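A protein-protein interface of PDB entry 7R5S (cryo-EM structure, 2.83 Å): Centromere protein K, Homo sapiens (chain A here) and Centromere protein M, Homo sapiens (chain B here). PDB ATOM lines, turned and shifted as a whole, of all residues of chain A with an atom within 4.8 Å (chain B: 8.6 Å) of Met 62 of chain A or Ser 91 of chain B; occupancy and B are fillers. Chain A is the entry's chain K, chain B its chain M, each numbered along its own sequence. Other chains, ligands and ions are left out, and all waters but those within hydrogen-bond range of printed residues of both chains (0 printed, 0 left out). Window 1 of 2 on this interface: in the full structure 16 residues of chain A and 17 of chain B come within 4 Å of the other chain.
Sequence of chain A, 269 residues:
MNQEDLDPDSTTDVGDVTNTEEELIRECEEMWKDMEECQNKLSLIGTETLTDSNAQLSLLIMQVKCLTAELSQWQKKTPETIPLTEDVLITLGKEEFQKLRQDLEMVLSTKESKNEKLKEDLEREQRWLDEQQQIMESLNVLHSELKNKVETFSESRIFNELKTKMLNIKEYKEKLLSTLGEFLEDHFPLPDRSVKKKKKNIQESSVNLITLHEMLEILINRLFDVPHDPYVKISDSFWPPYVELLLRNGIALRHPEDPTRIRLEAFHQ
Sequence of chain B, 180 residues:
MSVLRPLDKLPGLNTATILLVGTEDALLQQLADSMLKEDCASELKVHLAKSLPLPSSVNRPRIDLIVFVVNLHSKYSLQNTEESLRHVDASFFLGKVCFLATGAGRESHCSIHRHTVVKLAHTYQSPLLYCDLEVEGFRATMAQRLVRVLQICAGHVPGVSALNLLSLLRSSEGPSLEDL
O of Met 62 of chain A lies close to SG of Cys 66 of chain A, at 3.5 Å.
Of the 9 printed residues of chain A, 4 touch a printed residue of chain B. Hydrophobic or aromatic side chains of chain A that line the printed part of chain B: Leu 59 and Met 62.
Among the printed residues, merely in contact across the chains: Leu 59 of chain A with Ala 90 of chain B, Leu 59 of chain A with Phe 93 of chain B, Met 62 of chain A with Ala 90 of chain B, Met 62 of chain A with Ser 91 of chain B, Gln 63 of chain A with Leu 94 of chain B, Gln 63 of chain A with Leu 166 of chain B, Cys 66 of chain A with Leu 94 of chain B and Cys 66 of chain A with Leu 163 of chain B.
Met 62 of chain A touches just these residues of chain B: Ala 90 (3.6 Å) and Ser 91 (3.9 Å). Of the printed residues of chain B, Cys 66 of chain A touches Leu 94 and Leu 163. Leu 7 of chain B touches none of the printed residues of chain A. Printed residues of chain A within 4 Å of Ala 90 of chain B: Leu 59 and Met 62. Of chain A, only Met 62 comes within 4 Å of Ser 91 of chain B. Of the printed residues of chain A, Phe 93 of chain B touches Leu 59. Ala 162 of chain B touches none of the printed residues of chain A. Of the printed residues of chain A, Leu 163 of chain B touches Cys 66. Printed residues of chain A within 4 Å of Leu 166 of chain B: Gln 63 (3.4 Å).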
ATOM      1  N   SER A  58      22.396 -24.595 -19.668  1.00  0.00           N
ATOM      2  CA  SER A  58      21.080 -24.476 -19.049  1.00  0.00           C
ATOM      3  C   SER A  58      21.144 -23.627 -17.786  1.00  0.00           C
ATOM      4  O   SER A  58      20.275 -22.776 -17.554  1.00  0.00           O
ATOM      5  CB  SER A  58      20.521 -25.864 -18.736  1.00  0.00           C
ATOM      6  OG  SER A  58      20.722 -26.750 -19.822  1.00  0.00           O
ATOM      7  N   LEU A  59      22.172 -23.837 -16.961  1.00  0.00           N
ATOM      8  CA  LEU A  59      22.309 -23.043 -15.747  1.00  0.00           C
ATOM      9  C   LEU A  59      22.592 -21.583 -16.071  1.00  0.00           C
ATOM     10  O   LEU A  59      22.107 -20.686 -15.375  1.00  0.00           O
ATOM     11  CB  LEU A  59      23.406 -23.626 -14.857  1.00  0.00           C
ATOM     12  CG  LEU A  59      23.029 -24.917 -14.126  1.00  0.00           C
ATOM     13  CD1 LEU A  59      24.185 -25.415 -13.278  1.00  0.00           C
ATOM     14  CD2 LEU A  59      21.787 -24.707 -13.275  1.00  0.00           C
ATOM     15  N   LEU A  60      23.356 -21.319 -17.135  1.00  0.00           N
ATOM     16  CA  LEU A  60      23.600 -19.935 -17.535  1.00  0.00           C
ATOM     17  C   LEU A  60      22.311 -19.253 -17.984  1.00  0.00           C
ATOM     18  O   LEU A  60      22.048 -18.098 -17.624  1.00  0.00           O
ATOM     19  CB  LEU A  60      24.650 -19.884 -18.643  1.00  0.00           C
ATOM     20  CG  LEU A  60      26.092 -20.188 -18.233  1.00  0.00           C
ATOM     21  CD1 LEU A  60      27.014 -20.143 -19.438  1.00  0.00           C
ATOM     22  CD2 LEU A  60      26.560 -19.217 -17.161  1.00  0.00           C
ATOM     23  N   ILE A  61      21.492 -19.956 -18.770  1.00  0.00           N
ATOM     24  CA  ILE A  61      20.218 -19.388 -19.212  1.00  0.00           C
ATOM     25  C   ILE A  61      19.308 -19.123 -18.017  1.00  0.00           C
ATOM     26  O   ILE A  61      18.650 -18.074 -17.934  1.00  0.00           O
ATOM     27  CB  ILE A  61      19.547 -20.316 -20.243  1.00  0.00           C
ATOM     28  CG1 ILE A  61      20.415 -20.436 -21.497  1.00  0.00           C
ATOM     29  CG2 ILE A  61      18.162 -19.806 -20.602  1.00  0.00           C
ATOM     30  CD1 ILE A  61      20.687 -19.116 -22.181  1.00  0.00           C
ATOM     31  N   MET A  62      19.256 -20.066 -17.073  1.00  0.00           N
ATOM     32  CA  MET A  62      18.432 -19.873 -15.885  1.00  0.00           C
ATOM     33  C   MET A  62      18.928 -18.698 -15.051  1.00  0.00           C
ATOM     34  O   MET A  62      18.124 -17.937 -14.499  1.00  0.00           O
ATOM     35  CB  MET A  62      18.402 -21.151 -15.048  1.00  0.00           C
ATOM     36  CG  MET A  62      17.636 -22.291 -15.694  1.00  0.00           C
ATOM     37  SD  MET A  62      17.377 -23.671 -14.566  1.00  0.00           S
ATOM     38  CE  MET A  62      16.415 -22.881 -13.280  1.00  0.00           C
ATOM     39  N   GLN A  63      20.250 -18.533 -14.950  1.00  0.00           N
ATOM     40  CA  GLN A  63      20.800 -17.392 -14.227  1.00  0.00           C
ATOM     41  C   GLN A  63      20.417 -16.082 -14.899  1.00  0.00           C
ATOM     42  O   GLN A  63      20.077 -15.105 -14.223  1.00  0.00           O
ATOM     43  CB  GLN A  63      22.320 -17.514 -14.126  1.00  0.00           C
ATOM     44  CG  GLN A  63      22.801 -18.551 -13.129  1.00  0.00           C
ATOM     45  CD  GLN A  63      24.302 -18.750 -13.180  1.00  0.00           C
ATOM     46  OE1 GLN A  63      25.036 -17.894 -13.670  1.00  0.00           O
ATOM     47  NE2 GLN A  63      24.764 -19.889 -12.677  1.00  0.00           N
ATOM     48  N   VAL A  64      20.469 -16.043 -16.232  1.00  0.00           N
ATOM     49  CA  VAL A  64      20.072 -14.836 -16.956  1.00  0.00           C
ATOM     50  C   VAL A  64      18.615 -14.501 -16.670  1.00  0.00           C
ATOM     51  O   VAL A  64      18.267 -13.351 -16.370  1.00  0.00           O
ATOM     52  CB  VAL A  64      20.327 -15.002 -18.464  1.00  0.00           C
ATOM     53  CG1 VAL A  64      19.623 -13.905 -19.245  1.00  0.00           C
ATOM     54  CG2 VAL A  64      21.812 -14.981 -18.748  1.00  0.00           C
ATOM     55  N   LYS A  65      17.738 -15.506 -16.751  1.00  0.00           N
ATOM     56  CA  LYS A  65      16.317 -15.269 -16.509  1.00  0.00           C
ATOM     57  C   LYS A  65      16.072 -14.788 -15.081  1.00  0.00           C
ATOM     58  O   LYS A  65      15.309 -13.841 -14.849  1.00  0.00           O
ATOM     59  CB  LYS A  65      15.517 -16.540 -16.793  1.00  0.00           C
ATOM     60  CG  LYS A  65      15.535 -16.970 -18.249  1.00  0.00           C
ATOM     61  CD  LYS A  65      14.697 -18.219 -18.463  1.00  0.00           C
ATOM     62  CE  LYS A  65      14.691 -18.636 -19.923  1.00  0.00           C
ATOM     63  NZ  LYS A  65      13.910 -19.884 -20.140  1.00  0.00           N
ATOM     64  N   CYS A  66      16.724 -15.428 -14.107  1.00  0.00           N
ATOM     65  CA  CYS A  66      16.521 -15.058 -12.712  1.00  0.00           C
ATOM     66  C   CYS A  66      17.043 -13.658 -12.416  1.00  0.00           C
ATOM     67  O   CYS A  66      16.407 -12.910 -11.666  1.00  0.00           O
ATOM     68  CB  CYS A  66      17.191 -16.082 -11.797  1.00  0.00           C
ATOM     69  SG  CYS A  66      16.252 -17.611 -11.593  1.00  0.00           S
ATOM     70  N   VAL B   3      12.078 -36.174  -7.018  1.00  0.00           N
ATOM     71  CA  VAL B   3      13.004 -35.078  -7.275  1.00  0.00           C
ATOM     72  C   VAL B   3      12.810 -34.022  -6.196  1.00  0.00           C
ATOM     73  O   VAL B   3      11.674 -33.647  -5.881  1.00  0.00           O
ATOM     74  CB  VAL B   3      12.794 -34.480  -8.677  1.00  0.00           C
ATOM     75  CG1 VAL B   3      13.806 -33.378  -8.943  1.00  0.00           C
ATOM     76  CG2 VAL B   3      12.895 -35.568  -9.733  1.00  0.00           C
ATOM     77  N   LEU B   4      13.917 -33.548  -5.630  1.00  0.00           N
ATOM     78  CA  LEU B   4      13.870 -32.548  -4.574  1.00  0.00           C
ATOM     79  C   LEU B   4      13.718 -31.156  -5.177  1.00  0.00           C
ATOM     80  O   LEU B   4      14.426 -30.802  -6.124  1.00  0.00           O
ATOM     81  CB  LEU B   4      15.135 -32.624  -3.720  1.00  0.00           C
ATOM     82  CG  LEU B   4      15.052 -32.089  -2.291  1.00  0.00           C
ATOM     83  CD1 LEU B   4      14.038 -32.881  -1.483  1.00  0.00           C
ATOM     84  CD2 LEU B   4      16.420 -32.137  -1.631  1.00  0.00           C
ATOM     85  N   ARG B   5      12.794 -30.368  -4.627  1.00  0.00           N
ATOM     86  CA  ARG B   5      12.546 -29.028  -5.127  1.00  0.00           C
ATOM     87  C   ARG B   5      12.757 -28.004  -4.015  1.00  0.00           C
ATOM     88  O   ARG B   5      12.347 -28.241  -2.873  1.00  0.00           O
ATOM     89  CB  ARG B   5      11.118 -28.902  -5.685  1.00  0.00           C
ATOM     90  CG  ARG B   5      10.923 -27.743  -6.653  1.00  0.00           C
ATOM     91  CD  ARG B   5       9.454 -27.424  -6.859  1.00  0.00           C
ATOM     92  NE  ARG B   5       8.704 -28.588  -7.319  1.00  0.00           N
ATOM     93  CZ  ARG B   5       8.388 -28.819  -8.590  1.00  0.00           C
ATOM     94  NH1 ARG B   5       8.754 -27.961  -9.532  1.00  0.00           N
ATOM     95  NH2 ARG B   5       7.703 -29.905  -8.917  1.00  0.00           N
ATOM     96  N   PRO B   6      13.396 -26.865  -4.314  1.00  0.00           N
ATOM     97  CA  PRO B   6      13.744 -25.906  -3.253  1.00  0.00           C
ATOM     98  C   PRO B   6      12.550 -25.269  -2.556  1.00  0.00           C
ATOM     99  O   PRO B   6      12.562 -25.110  -1.331  1.00  0.00           O
ATOM    100  CB  PRO B   6      14.568 -24.847  -3.998  1.00  0.00           C
ATOM    101  CG  PRO B   6      15.065 -25.535  -5.221  1.00  0.00           C
ATOM    102  CD  PRO B   6      13.984 -26.489  -5.609  1.00  0.00           C
ATOM    103  N   LEU B   7      11.520 -24.897  -3.312  1.00  0.00           N
ATOM    104  CA  LEU B   7      10.424 -24.083  -2.799  1.00  0.00           C
ATOM    105  C   LEU B   7       9.108 -24.851  -2.782  1.00  0.00           C
ATOM    106  O   LEU B   7       8.062 -24.336  -3.181  1.00  0.00           O
ATOM    107  CB  LEU B   7      10.282 -22.798  -3.613  1.00  0.00           C
ATOM    108  CG  LEU B   7      11.436 -21.798  -3.513  1.00  0.00           C
ATOM    109  CD1 LEU B   7      11.150 -20.565  -4.353  1.00  0.00           C
ATOM    110  CD2 LEU B   7      11.689 -21.415  -2.065  1.00  0.00           C
ATOM    111  N   VAL B  88      18.171 -34.062  -8.488  1.00  0.00           N
ATOM    112  CA  VAL B  88      17.853 -32.720  -8.022  1.00  0.00           C
ATOM    113  C   VAL B  88      17.581 -31.842  -9.234  1.00  0.00           C
ATOM    114  O   VAL B  88      18.251 -31.966 -10.264  1.00  0.00           O
ATOM    115  CB  VAL B  88      18.988 -32.125  -7.159  1.00  0.00           C
ATOM    116  CG1 VAL B  88      18.962 -32.724  -5.766  1.00  0.00           C
ATOM    117  CG2 VAL B  88      20.336 -32.361  -7.818  1.00  0.00           C
ATOM    118  N   ASP B  89      16.594 -30.961  -9.111  1.00  0.00           N
ATOM    119  CA  ASP B  89      16.238 -30.090 -10.219  1.00  0.00           C
ATOM    120  C   ASP B  89      17.282 -28.991 -10.397  1.00  0.00           C
ATOM    121  O   ASP B  89      18.082 -28.702  -9.502  1.00  0.00           O
ATOM    122  CB  ASP B  89      14.856 -29.477 -10.002  1.00  0.00           C
ATOM    123  CG  ASP B  89      14.708 -28.847  -8.634  1.00  0.00           C
ATOM    124  OD1 ASP B  89      15.667 -28.917  -7.837  1.00  0.00           O
ATOM    125  OD2 ASP B  89      13.631 -28.281  -8.355  1.00  0.00           O
ATOM    126  N   ALA B  90      17.268 -28.377 -11.582  1.00  0.00           N
ATOM    127  CA  ALA B  90      18.246 -27.339 -11.889  1.00  0.00           C
ATOM    128  C   ALA B  90      18.062 -26.110 -11.011  1.00  0.00           C
ATOM    129  O   ALA B  90      19.040 -25.422 -10.694  1.00  0.00           O
ATOM    130  CB  ALA B  90      18.154 -26.956 -13.366  1.00  0.00           C
ATOM    131  N   SER B  91      16.824 -25.824 -10.597  1.00  0.00           N
ATOM    132  CA  SER B  91      16.558 -24.644  -9.782  1.00  0.00           C
ATOM    133  C   SER B  91      17.263 -24.695  -8.433  1.00  0.00           C
ATOM    134  O   SER B  91      17.371 -23.663  -7.763  1.00  0.00           O
ATOM    135  CB  SER B  91      15.052 -24.481  -9.573  1.00  0.00           C
ATOM    136  OG  SER B  91      14.779 -23.686  -8.433  1.00  0.00           O
ATOM    137  N   PHE B  92      17.744 -25.869  -8.018  1.00  0.00           N
ATOM    138  CA  PHE B  92      18.482 -25.979  -6.768  1.00  0.00           C
ATOM    139  C   PHE B  92      19.943 -25.584  -6.918  1.00  0.00           C
ATOM    140  O   PHE B  92      20.609 -25.333  -5.908  1.00  0.00           O
ATOM    141  CB  PHE B  92      18.386 -27.408  -6.226  1.00  0.00           C
ATOM    142  CG  PHE B  92      18.032 -27.482  -4.768  1.00  0.00           C
ATOM    143  CD1 PHE B  92      17.069 -28.369  -4.321  1.00  0.00           C
ATOM    144  CD2 PHE B  92      18.659 -26.663  -3.845  1.00  0.00           C
ATOM    145  CE1 PHE B  92      16.739 -28.439  -2.982  1.00  0.00           C
ATOM    146  CE2 PHE B  92      18.334 -26.729  -2.505  1.00  0.00           C
ATOM    147  CZ  PHE B  92      17.372 -27.619  -2.073  1.00  0.00           C
ATOM    148  N   PHE B  93      20.456 -25.518  -8.146  1.00  0.00           N
ATOM    149  CA  PHE B  93      21.852 -25.184  -8.390  1.00  0.00           C
ATOM    150  C   PHE B  93      22.095 -23.683  -8.491  1.00  0.00           C
ATOM    151  O   PHE B  93      23.187 -23.272  -8.895  1.00  0.00           O
ATOM    152  CB  PHE B  93      22.342 -25.872  -9.667  1.00  0.00           C
ATOM    153  CG  PHE B  93      22.498 -27.358  -9.533  1.00  0.00           C
ATOM    154  CD1 PHE B  93      23.649 -27.900  -8.988  1.00  0.00           C
ATOM    155  CD2 PHE B  93      21.495 -28.214  -9.953  1.00  0.00           C
ATOM    156  CE1 PHE B  93      23.795 -29.267  -8.863  1.00  0.00           C
ATOM    157  CE2 PHE B  93      21.635 -29.581  -9.831  1.00  0.00           C
ATOM    158  CZ  PHE B  93      22.788 -30.110  -9.285  1.00  0.00           C
ATOM    159  N   LEU B  94      21.111 -22.861  -8.136  1.00  0.00           N
ATOM    160  CA  LEU B  94      21.254 -21.406  -8.203  1.00  0.00           C
ATOM    161  C   LEU B  94      21.691 -20.846  -6.848  1.00  0.00           C
ATOM    162  O   LEU B  94      21.014 -20.032  -6.221  1.00  0.00           O
ATOM    163  CB  LEU B  94      19.953 -20.770  -8.676  1.00  0.00           C
ATOM    164  CG  LEU B  94      19.499 -21.141 -10.088  1.00  0.00           C
ATOM    165  CD1 LEU B  94      18.182 -20.461 -10.424  1.00  0.00           C
ATOM    166  CD2 LEU B  94      20.565 -20.780 -11.109  1.00  0.00           C
ATOM    167  N   GLY B  95      22.856 -21.305  -6.400  1.00  0.00           N
ATOM    168  CA  GLY B  95      23.436 -20.825  -5.163  1.00  0.00           C
ATOM    169  C   GLY B  95      23.022 -21.566  -3.915  1.00  0.00           C
ATOM    170  O   GLY B  95      23.169 -21.022  -2.815  1.00  0.00           O
ATOM    171  N   LYS B  96      22.511 -22.792  -4.042  1.00  0.00           N
ATOM    172  CA  LYS B  96      22.081 -23.576  -2.890  1.00  0.00           C
ATOM    173  C   LYS B  96      22.774 -24.931  -2.807  1.00  0.00           C
ATOM    174  O   LYS B  96      22.336 -25.790  -2.034  1.00  0.00           O
ATOM    175  CB  LYS B  96      20.563 -23.772  -2.918  1.00  0.00           C
ATOM    176  CG  LYS B  96      19.761 -22.504  -2.675  1.00  0.00           C
ATOM    177  CD  LYS B  96      18.270 -22.770  -2.812  1.00  0.00           C
ATOM    178  CE  LYS B  96      17.449 -21.545  -2.449  1.00  0.00           C
ATOM    179  NZ  LYS B  96      17.600 -21.178  -1.015  1.00  0.00           N
ATOM    180  N   VAL B  97      23.839 -25.146  -3.575  1.00  0.00           N
ATOM    181  CA  VAL B  97      24.562 -26.412  -3.592  1.00  0.00           C
ATOM    182  C   VAL B  97      26.050 -26.126  -3.437  1.00  0.00           C
ATOM    183  O   VAL B  97      26.590 -25.226  -4.091  1.00  0.00           O
ATOM    184  CB  VAL B  97      24.291 -27.207  -4.888  1.00  0.00           C
ATOM    185  CG1 VAL B  97      25.192 -28.428  -4.969  1.00  0.00           C
ATOM    186  CG2 VAL B  97      22.831 -27.621  -4.961  1.00  0.00           C
ATOM    187  N   ALA B 162      20.542 -16.021  -2.144  1.00  0.00           N
ATOM    188  CA  ALA B 162      21.371 -17.075  -2.718  1.00  0.00           C
ATOM    189  C   ALA B 162      21.840 -16.707  -4.120  1.00  0.00           C
ATOM    190  O   ALA B 162      22.961 -17.049  -4.517  1.00  0.00           O
ATOM    191  CB  ALA B 162      20.605 -18.396  -2.736  1.00  0.00           C
ATOM    192  N   LEU B 163      20.997 -16.008  -4.884  1.00  0.00           N
ATOM    193  CA  LEU B 163      21.392 -15.583  -6.222  1.00  0.00           C
ATOM    194  C   LEU B 163      22.537 -14.580  -6.173  1.00  0.00           C
ATOM    195  O   LEU B 163      23.361 -14.532  -7.092  1.00  0.00           O
ATOM    196  CB  LEU B 163      20.191 -14.991  -6.958  1.00  0.00           C
ATOM    197  CG  LEU B 163      20.311 -14.860  -8.476  1.00  0.00           C
ATOM    198  CD1 LEU B 163      20.618 -16.208  -9.107  1.00  0.00           C
ATOM    199  CD2 LEU B 163      19.040 -14.271  -9.061  1.00  0.00           C
ATOM    200  N   LEU B 166      25.696 -16.510  -5.372  1.00  0.00           N
ATOM    201  CA  LEU B 166      26.206 -17.150  -6.579  1.00  0.00           C
ATOM    202  C   LEU B 166      27.190 -16.245  -7.310  1.00  0.00           C
ATOM    203  O   LEU B 166      28.167 -16.722  -7.897  1.00  0.00           O
ATOM    204  CB  LEU B 166      25.045 -17.535  -7.495  1.00  0.00           C
ATOM    205  CG  LEU B 166      25.393 -18.267  -8.791  1.00  0.00           C
ATOM    206  CD1 LEU B 166      26.049 -19.604  -8.493  1.00  0.00           C
ATOM    207  CD2 LEU B 166      24.150 -18.453  -9.641  1.00  0.00           C
